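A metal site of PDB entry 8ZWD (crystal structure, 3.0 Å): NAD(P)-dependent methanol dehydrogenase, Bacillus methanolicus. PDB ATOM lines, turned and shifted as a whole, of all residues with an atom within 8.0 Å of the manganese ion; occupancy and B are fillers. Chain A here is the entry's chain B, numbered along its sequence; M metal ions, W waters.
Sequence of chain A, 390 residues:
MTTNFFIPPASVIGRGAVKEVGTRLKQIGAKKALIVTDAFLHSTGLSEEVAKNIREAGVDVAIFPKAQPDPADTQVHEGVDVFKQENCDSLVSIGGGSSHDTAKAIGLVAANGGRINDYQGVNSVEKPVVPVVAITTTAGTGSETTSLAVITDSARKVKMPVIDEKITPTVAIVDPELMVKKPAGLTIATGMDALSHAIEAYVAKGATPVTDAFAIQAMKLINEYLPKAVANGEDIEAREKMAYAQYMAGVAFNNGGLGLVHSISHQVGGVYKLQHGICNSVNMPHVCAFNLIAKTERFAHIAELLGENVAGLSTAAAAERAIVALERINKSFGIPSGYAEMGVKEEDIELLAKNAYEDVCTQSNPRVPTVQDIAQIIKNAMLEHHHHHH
A ring nitrogen (NE2) of His 262 sits close to the side-chain amide nitrogen of Asn 280, at 3.3 Å.
The backbone carbonyl oxygen (O) of His 262 lies within hydrogen-bond range of a ring nitrogen (ND1) of His 266 (2.9 Å).
The side-chain carboxylate of Glu 200 is in hydrogen-bond range of a ring nitrogen (ND1) of His 262.
The side-chain amide oxygen (OD1) of Asn 280 lies close to the backbone carbonyl oxygen (O) of His 276, at 3.3 Å.
OD1 of Asp 193 lies close to ND2 of Asn 280 (2.6 Å).
The manganese ion is bound by NE2 of His 197.
The manganese ion is bound by a ring nitrogen (NE2) of His 262, 2.3 Å away.
NE2 of His 276 is bound to the manganese ion.
The manganese ion is bound by OD1 of Asp 193 (2.4 Å).
OD2 of Asp 193 is bound to the manganese ion, at 2.5 Å.
The manganese ion has five donor atoms within binding distance.
Within 4 Å of the manganese ion: Asp 193, His 197, His 262 and His 276.
The nearest printed residue that does not touch the manganese ion is Asn 280 (4.04 Å).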
ATOM      1  N   GLY A 140      22.550  21.185  29.344  1.00  0.00           N
ATOM      2  CA  GLY A 140      23.361  22.353  29.034  1.00  0.00           C
ATOM      3  C   GLY A 140      24.524  22.424  29.997  1.00  0.00           C
ATOM      4  O   GLY A 140      24.693  21.554  30.855  1.00  0.00           O
ATOM      5  N   THR A 141      25.323  23.475  29.846  1.00  0.00           N
ATOM      6  CA  THR A 141      26.537  23.739  30.634  1.00  0.00           C
ATOM      7  C   THR A 141      27.667  22.777  30.278  1.00  0.00           C
ATOM      8  O   THR A 141      28.789  23.216  30.015  1.00  0.00           O
ATOM      9  CB  THR A 141      26.283  23.698  32.164  1.00  0.00           C
ATOM     10  OG1 THR A 141      26.015  22.350  32.587  1.00  0.00           O
ATOM     11  CG2 THR A 141      25.110  24.586  32.548  1.00  0.00           C
ATOM     12  N   GLY A 142      27.392  21.477  30.254  1.00  0.00           N
ATOM     13  CA  GLY A 142      28.445  20.503  30.039  1.00  0.00           C
ATOM     14  C   GLY A 142      29.554  20.555  31.066  1.00  0.00           C
ATOM     15  O   GLY A 142      30.666  20.088  30.808  1.00  0.00           O
ATOM     16  N   SER A 143      29.263  21.101  32.256  1.00  0.00           N
ATOM     17  CA  SER A 143      30.298  21.267  33.261  1.00  0.00           C
ATOM     18  C   SER A 143      30.825  19.940  33.778  1.00  0.00           C
ATOM     19  O   SER A 143      31.880  19.923  34.426  1.00  0.00           O
ATOM     20  CB  SER A 143      29.755  22.097  34.426  1.00  0.00           C
ATOM     21  OG  SER A 143      29.148  23.287  33.935  1.00  0.00           O
ATOM     22  N   LEU A 148      36.448  24.220  34.039  1.00  0.00           N
ATOM     23  CA  LEU A 148      36.079  25.595  34.330  1.00  0.00           C
ATOM     24  C   LEU A 148      34.939  25.645  35.335  1.00  0.00           C
ATOM     25  O   LEU A 148      34.038  24.807  35.299  1.00  0.00           O
ATOM     26  CB  LEU A 148      35.661  26.317  33.031  1.00  0.00           C
ATOM     27  CG  LEU A 148      34.699  27.497  33.132  1.00  0.00           C
ATOM     28  CD1 LEU A 148      35.375  28.687  33.785  1.00  0.00           C
ATOM     29  CD2 LEU A 148      34.129  27.866  31.764  1.00  0.00           C
ATOM     30  N   VAL A 150      32.355  28.808  37.083  1.00  0.00           N
ATOM     31  CA  VAL A 150      31.960  30.217  37.038  1.00  0.00           C
ATOM     32  C   VAL A 150      31.297  30.540  38.364  1.00  0.00           C
ATOM     33  O   VAL A 150      30.128  30.214  38.597  1.00  0.00           O
ATOM     34  CB  VAL A 150      31.038  30.520  35.849  1.00  0.00           C
ATOM     35  CG1 VAL A 150      30.888  32.007  35.661  1.00  0.00           C
ATOM     36  CG2 VAL A 150      31.594  29.892  34.581  1.00  0.00           C
ATOM     37  N   ALA A 189      16.619  27.347  28.225  1.00  0.00           N
ATOM     38  CA  ALA A 189      17.825  27.996  28.742  1.00  0.00           C
ATOM     39  C   ALA A 189      19.059  27.134  28.540  1.00  0.00           C
ATOM     40  O   ALA A 189      20.045  27.550  27.918  1.00  0.00           O
ATOM     41  CB  ALA A 189      17.633  28.339  30.215  1.00  0.00           C
ATOM     42  N   THR A 190      19.029  25.904  29.071  1.00  0.00           N
ATOM     43  CA  THR A 190      20.185  25.016  29.004  1.00  0.00           C
ATOM     44  C   THR A 190      20.535  24.629  27.568  1.00  0.00           C
ATOM     45  O   THR A 190      21.716  24.526  27.220  1.00  0.00           O
ATOM     46  CB  THR A 190      19.922  23.761  29.840  1.00  0.00           C
ATOM     47  OG1 THR A 190      18.698  23.158  29.413  1.00  0.00           O
ATOM     48  CG2 THR A 190      19.818  24.111  31.311  1.00  0.00           C
ATOM     49  N   MET A 192      19.917  26.407  24.836  1.00  0.00           N
ATOM     50  CA  MET A 192      20.515  27.561  24.206  1.00  0.00           C
ATOM     51  C   MET A 192      21.923  27.802  24.727  1.00  0.00           C
ATOM     52  O   MET A 192      22.775  28.301  23.977  1.00  0.00           O
ATOM     53  CB  MET A 192      19.636  28.792  24.414  1.00  0.00           C
ATOM     54  CG  MET A 192      18.340  28.755  23.627  1.00  0.00           C
ATOM     55  SD  MET A 192      18.599  28.654  21.839  1.00  0.00           S
ATOM     56  CE  MET A 192      19.621  30.094  21.573  1.00  0.00           C
ATOM     57  N   ASP A 193      22.207  27.459  25.979  1.00  0.00           N
ATOM     58  CA  ASP A 193      23.591  27.535  26.443  1.00  0.00           C
ATOM     59  C   ASP A 193      24.452  26.503  25.728  1.00  0.00           C
ATOM     60  O   ASP A 193      25.606  26.760  25.395  1.00  0.00           O
ATOM     61  CB  ASP A 193      23.687  27.357  27.960  1.00  0.00           C
ATOM     62  CG  ASP A 193      25.022  27.827  28.537  1.00  0.00           C
ATOM     63  OD1 ASP A 193      25.605  28.826  28.028  1.00  0.00           O
ATOM     64  OD2 ASP A 193      25.491  27.202  29.512  1.00  0.00           O
ATOM     65  N   ALA A 194      23.871  25.335  25.445  1.00  0.00           N
ATOM     66  CA  ALA A 194      24.587  24.335  24.663  1.00  0.00           C
ATOM     67  C   ALA A 194      24.918  24.853  23.274  1.00  0.00           C
ATOM     68  O   ALA A 194      26.062  24.753  22.805  1.00  0.00           O
ATOM     69  CB  ALA A 194      23.748  23.054  24.580  1.00  0.00           C
ATOM     70  N   SER A 196      25.067  27.928  22.324  1.00  0.00           N
ATOM     71  CA  SER A 196      26.060  28.965  22.577  1.00  0.00           C
ATOM     72  C   SER A 196      27.464  28.365  22.604  1.00  0.00           C
ATOM     73  O   SER A 196      28.353  28.794  21.850  1.00  0.00           O
ATOM     74  CB  SER A 196      25.712  29.658  23.899  1.00  0.00           C
ATOM     75  OG  SER A 196      26.606  30.698  24.216  1.00  0.00           O
ATOM     76  N   HIS A 197      27.672  27.362  23.466  1.00  0.00           N
ATOM     77  CA  HIS A 197      28.980  26.744  23.614  1.00  0.00           C
ATOM     78  C   HIS A 197      29.509  26.224  22.284  1.00  0.00           C
ATOM     79  O   HIS A 197      30.674  26.455  21.938  1.00  0.00           O
ATOM     80  CB  HIS A 197      28.907  25.595  24.625  1.00  0.00           C
ATOM     81  CG  HIS A 197      28.588  26.027  26.014  1.00  0.00           C
ATOM     82  ND1 HIS A 197      28.215  25.156  27.010  1.00  0.00           N
ATOM     83  CD2 HIS A 197      28.594  27.267  26.574  1.00  0.00           C
ATOM     84  CE1 HIS A 197      28.005  25.826  28.125  1.00  0.00           C
ATOM     85  NE2 HIS A 197      28.226  27.110  27.892  1.00  0.00           N
ATOM     86  N   GLU A 200      30.330  29.010  19.718  1.00  0.00           N
ATOM     87  CA  GLU A 200      31.507  29.757  20.138  1.00  0.00           C
ATOM     88  C   GLU A 200      32.771  28.917  20.012  1.00  0.00           C
ATOM     89  O   GLU A 200      33.822  29.430  19.609  1.00  0.00           O
ATOM     90  CB  GLU A 200      31.326  30.241  21.573  1.00  0.00           C
ATOM     91  CG  GLU A 200      30.373  31.395  21.683  1.00  0.00           C
ATOM     92  CD  GLU A 200      30.849  32.446  22.653  1.00  0.00           C
ATOM     93  OE1 GLU A 200      31.157  32.081  23.811  1.00  0.00           O
ATOM     94  OE2 GLU A 200      30.912  33.630  22.261  1.00  0.00           O
ATOM     95  N   PHE A 253      34.087  23.647  23.836  1.00  0.00           N
ATOM     96  CA  PHE A 253      34.462  24.975  24.320  1.00  0.00           C
ATOM     97  C   PHE A 253      35.562  24.900  25.367  1.00  0.00           C
ATOM     98  O   PHE A 253      36.383  25.824  25.460  1.00  0.00           O
ATOM     99  CB  PHE A 253      33.250  25.764  24.844  1.00  0.00           C
ATOM    100  CG  PHE A 253      32.907  25.511  26.296  1.00  0.00           C
ATOM    101  CD1 PHE A 253      33.651  26.078  27.321  1.00  0.00           C
ATOM    102  CD2 PHE A 253      31.805  24.744  26.626  1.00  0.00           C
ATOM    103  CE1 PHE A 253      33.322  25.848  28.643  1.00  0.00           C
ATOM    104  CE2 PHE A 253      31.467  24.523  27.944  1.00  0.00           C
ATOM    105  CZ  PHE A 253      32.221  25.080  28.951  1.00  0.00           C
ATOM    106  N   LEU A 258      35.631  29.856  24.395  1.00  0.00           N
ATOM    107  CA  LEU A 258      34.355  30.539  24.329  1.00  0.00           C
ATOM    108  C   LEU A 258      34.550  31.891  23.662  1.00  0.00           C
ATOM    109  O   LEU A 258      35.390  32.036  22.766  1.00  0.00           O
ATOM    110  CB  LEU A 258      33.751  30.688  25.725  1.00  0.00           C
ATOM    111  CG  LEU A 258      33.136  29.404  26.321  1.00  0.00           C
ATOM    112  CD1 LEU A 258      32.841  29.578  27.792  1.00  0.00           C
ATOM    113  CD2 LEU A 258      31.873  28.984  25.564  1.00  0.00           C
ATOM    114  N   VAL A 261      30.044  36.096  23.839  1.00  0.00           N
ATOM    115  CA  VAL A 261      28.722  35.746  24.352  1.00  0.00           C
ATOM    116  C   VAL A 261      28.790  35.512  25.845  1.00  0.00           C
ATOM    117  O   VAL A 261      28.079  36.145  26.638  1.00  0.00           O
ATOM    118  CB  VAL A 261      28.152  34.517  23.608  1.00  0.00           C
ATOM    119  CG1 VAL A 261      26.932  33.995  24.336  1.00  0.00           C
ATOM    120  CG2 VAL A 261      27.801  34.900  22.180  1.00  0.00           C
ATOM    121  N   HIS A 262      29.686  34.632  26.270  1.00  0.00           N
ATOM    122  CA  HIS A 262      29.801  34.349  27.697  1.00  0.00           C
ATOM    123  C   HIS A 262      30.430  35.511  28.442  1.00  0.00           C
ATOM    124  O   HIS A 262      30.070  35.761  29.593  1.00  0.00           O
ATOM    125  CB  HIS A 262      30.575  33.047  27.905  1.00  0.00           C
ATOM    126  CG  HIS A 262      29.733  31.839  27.684  1.00  0.00           C
ATOM    127  ND1 HIS A 262      29.194  31.519  26.461  1.00  0.00           N
ATOM    128  CD2 HIS A 262      29.291  30.887  28.547  1.00  0.00           C
ATOM    129  CE1 HIS A 262      28.464  30.421  26.573  1.00  0.00           C
ATOM    130  NE2 HIS A 262      28.506  30.018  27.829  1.00  0.00           N
ATOM    131  N   SER A 265      27.510  37.780  28.994  1.00  0.00           N
ATOM    132  CA  SER A 265      26.513  37.195  29.877  1.00  0.00           C
ATOM    133  C   SER A 265      27.009  37.085  31.301  1.00  0.00           C
ATOM    134  O   SER A 265      26.210  37.102  32.237  1.00  0.00           O
ATOM    135  CB  SER A 265      26.068  35.811  29.380  1.00  0.00           C
ATOM    136  OG  SER A 265      25.394  35.885  28.128  1.00  0.00           O
ATOM    137  N   HIS A 266      28.331  36.989  31.504  1.00  0.00           N
ATOM    138  CA  HIS A 266      28.845  36.893  32.863  1.00  0.00           C
ATOM    139  C   HIS A 266      28.598  38.179  33.639  1.00  0.00           C
ATOM    140  O   HIS A 266      28.165  38.136  34.787  1.00  0.00           O
ATOM    141  CB  HIS A 266      30.328  36.524  32.834  1.00  0.00           C
ATOM    142  CG  HIS A 266      30.576  35.094  32.458  1.00  0.00           C
ATOM    143  ND1 HIS A 266      31.681  34.675  31.753  1.00  0.00           N
ATOM    144  CD2 HIS A 266      29.825  33.984  32.672  1.00  0.00           C
ATOM    145  CE1 HIS A 266      31.603  33.375  31.548  1.00  0.00           C
ATOM    146  NE2 HIS A 266      30.501  32.927  32.102  1.00  0.00           N
ATOM    147  N   HIS A 276      21.488  32.272  32.617  1.00  0.00           N
ATOM    148  CA  HIS A 276      22.648  32.313  31.730  1.00  0.00           C
ATOM    149  C   HIS A 276      22.278  32.027  30.281  1.00  0.00           C
ATOM    150  O   HIS A 276      22.724  32.737  29.355  1.00  0.00           O
ATOM    151  CB  HIS A 276      23.678  31.309  32.257  1.00  0.00           C
ATOM    152  CG  HIS A 276      24.888  31.142  31.385  1.00  0.00           C
ATOM    153  ND1 HIS A 276      25.725  32.177  31.061  1.00  0.00           N
ATOM    154  CD2 HIS A 276      25.395  30.036  30.791  1.00  0.00           C
ATOM    155  CE1 HIS A 276      26.701  31.726  30.293  1.00  0.00           C
ATOM    156  NE2 HIS A 276      26.528  30.426  30.116  1.00  0.00           N
ATOM    157  N   GLY A 277      21.469  30.993  30.051  1.00  0.00           N
ATOM    158  CA  GLY A 277      21.117  30.622  28.686  1.00  0.00           C
ATOM    159  C   GLY A 277      20.373  31.723  27.956  1.00  0.00           C
ATOM    160  O   GLY A 277      20.626  31.971  26.774  1.00  0.00           O
ATOM    161  N   ASN A 280      22.688  34.547  27.020  1.00  0.00           N
ATOM    162  CA  ASN A 280      23.445  34.093  25.860  1.00  0.00           C
ATOM    163  C   ASN A 280      22.622  34.215  24.581  1.00  0.00           C
ATOM    164  O   ASN A 280      23.152  34.597  23.536  1.00  0.00           O
ATOM    165  CB  ASN A 280      23.889  32.652  26.045  1.00  0.00           C
ATOM    166  CG  ASN A 280      25.001  32.522  27.033  1.00  0.00           C
ATOM    167  OD1 ASN A 280      25.417  33.511  27.629  1.00  0.00           O
ATOM    168  ND2 ASN A 280      25.487  31.305  27.215  1.00  0.00           N
HETATM  169 MN    MN M   1      27.590  28.530  29.271  1.00  0.00          MN
HETATM  170  O   HOH W   1      28.869  27.399  31.902  1.00  0.00           O
